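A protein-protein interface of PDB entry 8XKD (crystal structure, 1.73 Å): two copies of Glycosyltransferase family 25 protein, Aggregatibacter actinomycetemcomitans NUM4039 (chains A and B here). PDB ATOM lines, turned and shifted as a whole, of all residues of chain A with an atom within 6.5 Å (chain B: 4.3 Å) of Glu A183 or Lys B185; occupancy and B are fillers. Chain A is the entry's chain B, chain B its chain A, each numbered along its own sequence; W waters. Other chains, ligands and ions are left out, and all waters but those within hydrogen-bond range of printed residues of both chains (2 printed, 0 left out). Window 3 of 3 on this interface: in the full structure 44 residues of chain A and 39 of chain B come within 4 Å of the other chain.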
ATOM      1  N   GLN A  62     -22.830 -10.980  25.061  1.00  0.00           N
ATOM      2  CA  GLN A  62     -22.547 -10.277  23.802  1.00  0.00           C
ATOM      3  C   GLN A  62     -23.769  -9.704  23.063  1.00  0.00           C
ATOM      4  O   GLN A  62     -23.607  -8.950  22.096  1.00  0.00           O
ATOM      5  CB  GLN A  62     -21.722 -11.165  22.859  1.00  0.00           C
ATOM      6  CG  GLN A  62     -22.416 -12.414  22.322  1.00  0.00           C
ATOM      7  CD  GLN A  62     -22.292 -13.644  23.215  1.00  0.00           C
ATOM      8  OE1 GLN A  62     -22.254 -13.557  24.442  1.00  0.00           O
ATOM      9  NE2 GLN A  62     -22.267 -14.807  22.587  1.00  0.00           N
ATOM     10  N   LYS A 178     -29.586 -25.189  19.965  1.00  0.00           N
ATOM     11  CA  LYS A 178     -28.308 -25.947  20.024  1.00  0.00           C
ATOM     12  C   LYS A 178     -27.081 -25.056  20.110  1.00  0.00           C
ATOM     13  O   LYS A 178     -26.030 -25.510  20.559  1.00  0.00           O
ATOM     14  CB  LYS A 178     -28.183 -26.870  18.813  1.00  0.00           C
ATOM     15  CG  LYS A 178     -28.995 -28.146  18.959  1.00  0.00           C
ATOM     16  CD  LYS A 178     -28.572 -29.213  17.979  1.00  0.00           C
ATOM     17  CE  LYS A 178     -28.876 -28.810  16.548  1.00  0.00           C
ATOM     18  NZ  LYS A 178     -28.419 -29.831  15.569  1.00  0.00           N
ATOM     19  N   LEU A 179     -27.189 -23.799  19.685  1.00  0.00           N
ATOM     20  CA  LEU A 179     -26.048 -22.895  19.731  1.00  0.00           C
ATOM     21  C   LEU A 179     -25.520 -22.719  21.144  1.00  0.00           C
ATOM     22  O   LEU A 179     -26.290 -22.572  22.105  1.00  0.00           O
ATOM     23  CB  LEU A 179     -26.401 -21.519  19.183  1.00  0.00           C
ATOM     24  CG  LEU A 179     -26.702 -21.416  17.705  1.00  0.00           C
ATOM     25  CD1 LEU A 179     -27.237 -20.013  17.437  1.00  0.00           C
ATOM     26  CD2 LEU A 179     -25.496 -21.762  16.865  1.00  0.00           C
ATOM     27  N   THR A 180     -24.186 -22.737  21.279  1.00  0.00           N
ATOM     28  CA  THR A 180     -23.592 -22.522  22.586  1.00  0.00           C
ATOM     29  C   THR A 180     -23.551 -21.031  22.874  1.00  0.00           C
ATOM     30  O   THR A 180     -23.683 -20.204  21.969  1.00  0.00           O
ATOM     31  CB  THR A 180     -22.155 -23.069  22.661  1.00  0.00           C
ATOM     32  OG1 THR A 180     -21.324 -22.299  21.786  1.00  0.00           O
ATOM     33  CG2 THR A 180     -22.125 -24.551  22.246  1.00  0.00           C
ATOM     34  N   THR A 181     -23.333 -20.677  24.134  1.00  0.00           N
ATOM     35  CA  THR A 181     -23.260 -19.272  24.494  1.00  0.00           C
ATOM     36  C   THR A 181     -22.203 -18.550  23.642  1.00  0.00           C
ATOM     37  O   THR A 181     -22.455 -17.458  23.142  1.00  0.00           O
ATOM     38  CB  THR A 181     -23.059 -19.078  25.996  1.00  0.00           C
ATOM     39  OG1 THR A 181     -24.238 -19.538  26.676  1.00  0.00           O
ATOM     40  CG2 THR A 181     -22.869 -17.612  26.333  1.00  0.00           C
ATOM     41  N   GLU A 182     -21.062 -19.191  23.424  1.00  0.00           N
ATOM     42  CA  GLU A 182     -19.993 -18.625  22.593  1.00  0.00           C
ATOM     43  C   GLU A 182     -20.443 -18.374  21.153  1.00  0.00           C
ATOM     44  O   GLU A 182     -19.946 -17.455  20.507  1.00  0.00           O
ATOM     45  CB  GLU A 182     -18.758 -19.569  22.609  1.00  0.00           C
ATOM     46  CG  GLU A 182     -17.524 -19.083  21.850  1.00  0.00           C
ATOM     47  CD  GLU A 182     -17.602 -19.227  20.330  1.00  0.00           C
ATOM     48  OE1 GLU A 182     -18.194 -20.203  19.810  1.00  0.00           O
ATOM     49  OE2 GLU A 182     -17.080 -18.344  19.625  1.00  0.00           O
ATOM     50  N   GLU A 183     -21.346 -19.206  20.632  1.00  0.00           N
ATOM     51  CA  GLU A 183     -21.782 -19.100  19.232  1.00  0.00           C
ATOM     52  C   GLU A 183     -22.906 -18.101  19.019  1.00  0.00           C
ATOM     53  O   GLU A 183     -23.166 -17.713  17.872  1.00  0.00           O
ATOM     54  CB  GLU A 183     -22.233 -20.456  18.700  1.00  0.00           C
ATOM     55  CG  GLU A 183     -21.130 -21.481  18.645  1.00  0.00           C
ATOM     56  CD  GLU A 183     -21.622 -22.838  18.228  1.00  0.00           C
ATOM     57  OE1 GLU A 183     -22.682 -23.295  18.725  1.00  0.00           O
ATOM     58  OE2 GLU A 183     -20.929 -23.456  17.395  1.00  0.00           O
ATOM     59  N   ILE A 184     -23.547 -17.668  20.097  1.00  0.00           N
ATOM     60  CA  ILE A 184     -24.674 -16.744  19.945  1.00  0.00           C
ATOM     61  C   ILE A 184     -24.207 -15.414  19.350  1.00  0.00           C
ATOM     62  O   ILE A 184     -23.195 -14.841  19.775  1.00  0.00           O
ATOM     63  CB  ILE A 184     -25.369 -16.449  21.280  1.00  0.00           C
ATOM     64  CG1 ILE A 184     -25.960 -17.703  21.915  1.00  0.00           C
ATOM     65  CG2 ILE A 184     -26.482 -15.441  21.080  1.00  0.00           C
ATOM     66  CD1 ILE A 184     -26.767 -18.583  20.996  1.00  0.00           C
ATOM     67  N   LYS A 185     -24.961 -14.938  18.361  1.00  0.00           N
ATOM     68  CA  LYS A 185     -24.782 -13.642  17.756  1.00  0.00           C
ATOM     69  C   LYS A 185     -26.183 -13.058  17.513  1.00  0.00           C
ATOM     70  O   LYS A 185     -27.165 -13.773  17.624  1.00  0.00           O
ATOM     71  CB  LYS A 185     -24.032 -13.785  16.438  1.00  0.00           C
ATOM     72  CG  LYS A 185     -22.586 -14.172  16.633  1.00  0.00           C
ATOM     73  CD  LYS A 185     -21.864 -14.497  15.339  1.00  0.00           C
ATOM     74  CE  LYS A 185     -20.375 -14.644  15.621  1.00  0.00           C
ATOM     75  NZ  LYS A 185     -20.059 -15.389  16.883  1.00  0.00           N
ATOM     76  N   ILE A 190     -26.631 -14.701  12.456  1.00  0.00           N
ATOM     77  CA  ILE A 190     -26.773 -16.152  12.329  1.00  0.00           C
ATOM     78  C   ILE A 190     -27.486 -16.495  11.019  1.00  0.00           C
ATOM     79  O   ILE A 190     -27.001 -17.278  10.198  1.00  0.00           O
ATOM     80  CB  ILE A 190     -27.573 -16.771  13.497  1.00  0.00           C
ATOM     81  CG1 ILE A 190     -26.868 -16.528  14.840  1.00  0.00           C
ATOM     82  CG2 ILE A 190     -27.815 -18.259  13.244  1.00  0.00           C
ATOM     83  CD1 ILE A 190     -25.458 -17.108  14.903  1.00  0.00           C
ATOM     84  N   GLN A 194     -23.542 -16.323   9.108  1.00  0.00           N
ATOM     85  CA  GLN A 194     -22.932 -17.550   9.615  1.00  0.00           C
ATOM     86  C   GLN A 194     -23.504 -18.782   8.949  1.00  0.00           C
ATOM     87  O   GLN A 194     -22.754 -19.628   8.441  1.00  0.00           O
ATOM     88  CB  GLN A 194     -23.123 -17.681  11.133  1.00  0.00           C
ATOM     89  CG  GLN A 194     -22.335 -16.699  12.007  1.00  0.00           C
ATOM     90  CD  GLN A 194     -20.850 -16.577  11.656  1.00  0.00           C
ATOM     91  OE1 GLN A 194     -20.009 -17.383  12.082  1.00  0.00           O
ATOM     92  NE2 GLN A 194     -20.518 -15.536  10.890  1.00  0.00           N
ATOM     93  N   LEU B  63     -13.846 -29.288   9.207  1.00  0.00           N
ATOM     94  CA  LEU B  63     -12.720 -28.756   8.436  1.00  0.00           C
ATOM     95  C   LEU B  63     -12.028 -29.857   7.658  1.00  0.00           C
ATOM     96  O   LEU B  63     -11.890 -30.970   8.145  1.00  0.00           O
ATOM     97  CB  LEU B  63     -11.683 -28.093   9.365  1.00  0.00           C
ATOM     98  CG  LEU B  63     -11.893 -26.617   9.732  1.00  0.00           C
ATOM     99  CD1 LEU B  63     -13.248 -26.339  10.351  1.00  0.00           C
ATOM    100  CD2 LEU B  63     -10.794 -26.144  10.685  1.00  0.00           C
ATOM    101  N   GLU B 182     -17.020 -28.552  18.377  1.00  0.00           N
ATOM    102  CA  GLU B 182     -18.214 -28.142  17.639  1.00  0.00           C
ATOM    103  C   GLU B 182     -18.130 -26.669  17.202  1.00  0.00           C
ATOM    104  O   GLU B 182     -18.665 -26.305  16.149  1.00  0.00           O
ATOM    105  CB  GLU B 182     -19.485 -28.369  18.465  1.00  0.00           C
ATOM    106  CG  GLU B 182     -20.790 -28.144  17.678  1.00  0.00           C
ATOM    107  CD  GLU B 182     -21.195 -26.667  17.521  1.00  0.00           C
ATOM    108  OE1 GLU B 182     -20.968 -25.871  18.449  1.00  0.00           O
ATOM    109  OE2 GLU B 182     -21.738 -26.294  16.449  1.00  0.00           O
ATOM    110  N   GLU B 183     -17.470 -25.843  18.006  1.00  0.00           N
ATOM    111  CA  GLU B 183     -17.328 -24.398  17.727  1.00  0.00           C
ATOM    112  C   GLU B 183     -16.222 -24.049  16.719  1.00  0.00           C
ATOM    113  O   GLU B 183     -16.132 -22.917  16.246  1.00  0.00           O
ATOM    114  CB  GLU B 183     -17.087 -23.622  19.015  1.00  0.00           C
ATOM    115  CG  GLU B 183     -18.220 -23.736  20.023  1.00  0.00           C
ATOM    116  CD  GLU B 183     -17.869 -23.312  21.432  1.00  0.00           C
ATOM    117  OE1 GLU B 183     -16.666 -23.129  21.780  1.00  0.00           O
ATOM    118  OE2 GLU B 183     -18.822 -23.171  22.237  1.00  0.00           O
ATOM    119  N   ILE B 184     -15.358 -24.998  16.397  1.00  0.00           N
ATOM    120  CA  ILE B 184     -14.314 -24.744  15.397  1.00  0.00           C
ATOM    121  C   ILE B 184     -14.922 -24.424  14.024  1.00  0.00           C
ATOM    122  O   ILE B 184     -15.868 -25.061  13.585  1.00  0.00           O
ATOM    123  CB  ILE B 184     -13.362 -25.943  15.271  1.00  0.00           C
ATOM    124  CG1 ILE B 184     -12.580 -26.100  16.578  1.00  0.00           C
ATOM    125  CG2 ILE B 184     -12.442 -25.843  14.054  1.00  0.00           C
ATOM    126  CD1 ILE B 184     -11.787 -24.868  16.973  1.00  0.00           C
ATOM    127  N   LYS B 185     -14.353 -23.408  13.386  1.00  0.00           N
ATOM    128  CA  LYS B 185     -14.660 -23.047  12.001  1.00  0.00           C
ATOM    129  C   LYS B 185     -13.340 -22.720  11.291  1.00  0.00           C
ATOM    130  O   LYS B 185     -12.314 -22.541  11.957  1.00  0.00           O
ATOM    131  CB  LYS B 185     -15.589 -21.826  11.990  1.00  0.00           C
ATOM    132  CG  LYS B 185     -16.955 -22.101  12.634  1.00  0.00           C
ATOM    133  CD  LYS B 185     -17.768 -20.835  12.845  1.00  0.00           C
ATOM    134  CE  LYS B 185     -19.230 -21.155  13.153  1.00  0.00           C
ATOM    135  NZ  LYS B 185     -19.483 -21.521  14.584  1.00  0.00           N
ATOM    136  N   PRO B 186     -13.362 -22.621   9.951  1.00  0.00           N
ATOM    137  CA  PRO B 186     -12.130 -22.257   9.255  1.00  0.00           C
ATOM    138  C   PRO B 186     -11.575 -20.937   9.766  1.00  0.00           C
ATOM    139  O   PRO B 186     -12.318 -20.075  10.264  1.00  0.00           O
ATOM    140  CB  PRO B 186     -12.574 -22.179   7.782  1.00  0.00           C
ATOM    141  CG  PRO B 186     -13.738 -23.128   7.712  1.00  0.00           C
ATOM    142  CD  PRO B 186     -14.457 -22.896   8.996  1.00  0.00           C
ATOM    143  N   ILE B 187     -10.255 -20.817   9.703  1.00  0.00           N
ATOM    144  CA  ILE B 187      -9.562 -19.699  10.281  1.00  0.00           C
ATOM    145  C   ILE B 187     -10.135 -18.339   9.836  1.00  0.00           C
ATOM    146  O   ILE B 187     -10.288 -17.441  10.657  1.00  0.00           O
ATOM    147  CB  ILE B 187      -8.036 -19.783  10.030  1.00  0.00           C
ATOM    148  CG1 ILE B 187      -7.348 -18.641  10.749  1.00  0.00           C
ATOM    149  CG2 ILE B 187      -7.679 -19.864   8.536  1.00  0.00           C
ATOM    150  CD1 ILE B 187      -5.843 -18.754  10.695  1.00  0.00           C
ATOM    151  N   GLU B 189     -13.152 -17.547   9.059  1.00  0.00           N
ATOM    152  CA  GLU B 189     -14.437 -17.306   9.698  1.00  0.00           C
ATOM    153  C   GLU B 189     -14.267 -16.853  11.144  1.00  0.00           C
ATOM    154  O   GLU B 189     -14.973 -15.963  11.604  1.00  0.00           O
ATOM    155  CB  GLU B 189     -15.328 -18.547   9.635  1.00  0.00           C
ATOM    156  CG  GLU B 189     -15.710 -18.957   8.221  1.00  0.00           C
ATOM    157  CD  GLU B 189     -16.460 -17.864   7.483  1.00  0.00           C
ATOM    158  OE1 GLU B 189     -17.256 -17.157   8.138  1.00  0.00           O
ATOM    159  OE2 GLU B 189     -16.262 -17.722   6.251  1.00  0.00           O
ATOM    160  N   ILE B 190     -13.299 -17.434  11.847  1.00  0.00           N
ATOM    161  CA  ILE B 190     -13.048 -17.049  13.227  1.00  0.00           C
ATOM    162  C   ILE B 190     -12.406 -15.670  13.285  1.00  0.00           C
ATOM    163  O   ILE B 190     -12.880 -14.786  14.020  1.00  0.00           O
ATOM    164  CB  ILE B 190     -12.172 -18.078  13.953  1.00  0.00           C
ATOM    165  CG1 ILE B 190     -12.888 -19.432  14.062  1.00  0.00           C
ATOM    166  CG2 ILE B 190     -11.801 -17.566  15.347  1.00  0.00           C
ATOM    167  CD1 ILE B 190     -14.231 -19.392  14.766  1.00  0.00           C
ATOM    168  N   GLN B 194     -16.938 -14.149  12.714  1.00  0.00           N
ATOM    169  CA  GLN B 194     -17.368 -14.437  14.079  1.00  0.00           C
ATOM    170  C   GLN B 194     -16.945 -13.358  15.053  1.00  0.00           C
ATOM    171  O   GLN B 194     -17.754 -12.787  15.783  1.00  0.00           O
ATOM    172  CB  GLN B 194     -16.740 -15.759  14.564  1.00  0.00           C
ATOM    173  CG  GLN B 194     -17.344 -17.019  13.985  1.00  0.00           C
ATOM    174  CD  GLN B 194     -18.407 -17.597  14.900  1.00  0.00           C
ATOM    175  OE1 GLN B 194     -19.591 -17.520  14.606  1.00  0.00           O
ATOM    176  NE2 GLN B 194     -17.987 -18.150  16.036  1.00  0.00           N
HETATM  177  O   HOH W   1     -19.849 -21.419  24.984  1.00  0.00           O
HETATM  178  O   HOH W   2     -17.652 -20.727  16.753  1.00  0.00           O
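Lys A178 touches none of the printed residues of chain B. Printed residues of chain B within 4 Å of Thr A180: Glu B183. Of chain B, only Glu B182, Glu B183 and Lys B185 come within 4 Å of Glu A183. Of the printed residues of chain B, Gln A194 touches Lys B185 and Gln B194. Printed residues of chain A within 4 Å of Glu B182: Glu A183 (2.6 Å). Of the printed residues of chain A, Lys B185 touches Glu A183 and Gln A194. The nearest printed residue of chain B that does not touch Glu A183 is Gln B194 (4.8 Å). The nearest printed residue of chain A that does not touch Lys B185 is Glu A182 (5.5 Å).
N of Thr A180 sits at hydrogen-bond distance from OE1 of Glu A183, 3.0 Å away. O of Glu B189 lies within hydrogen-bond range of N of Gln B194, at 2.9 Å.
Glu A182 touches Glu B183, and with the chains exchanged Glu A183 touches Glu B182. Glu A183 touches Lys B185, but with the chains exchanged Lys A185 does not touch Glu B183 (8.5 Å). Lys A185 touches Gln B194, and with the chains exchanged Gln A194 touches Lys B185. Gln B194 touches its own counterpart, Gln A194.
Water W2 lies within hydrogen-bond range of the side-chain amide nitrogen (NE2) of Gln B194 (2.7 Å), the backbone carbonyl oxygen (O) of Glu B183 (2.7 Å), the side-chain amino group (NZ) of Lys B185 (2.9 Å) and the side-chain carboxylate (OE1) of Glu A182 (3.1 Å). Water W1 lies within hydrogen-bond range of the backbone NH (N) of Glu A182 (3.0 Å) and the side-chain carboxylate (OE2) of Glu B183 (3.4 Å).
Glu B183 touches Glu A182. OE2 of Glu A182 touches NE2 of Gln B194, 3.7 Å away. Glu A183 touches Glu B183. OE1 of Gln A194 touches CE of Lys B185, at 3.998 Å.
Of the 10 printed residues of chain B, 4 touch a printed residue of chain A. Along chain B the printed residues that touch a printed residue of chain A span positions 182 to 194. Of the 11 printed residues of chain A, 5 touch a printed residue of chain B. Among the printed residues, 9 pairs touch across the chains.
NZ of Lys A185 sits close to OE1 of Gln B194. OE2 of Glu A183 lies close to OE1 of Glu B182 (2.6 Å). The side-chain carboxylate of Glu B183 sits at hydrogen-bond distance from the side-chain hydroxyl of Thr A180. The side-chain amide oxygen (OE1) of Gln B194 lies close to the side-chain amide oxygen (OE1) of Gln A194 (2.6 Å). The side-chain amino group of Lys B185 lies within salt-bridge range of the side-chain carboxylate of Glu A183, 3.7 Å away.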
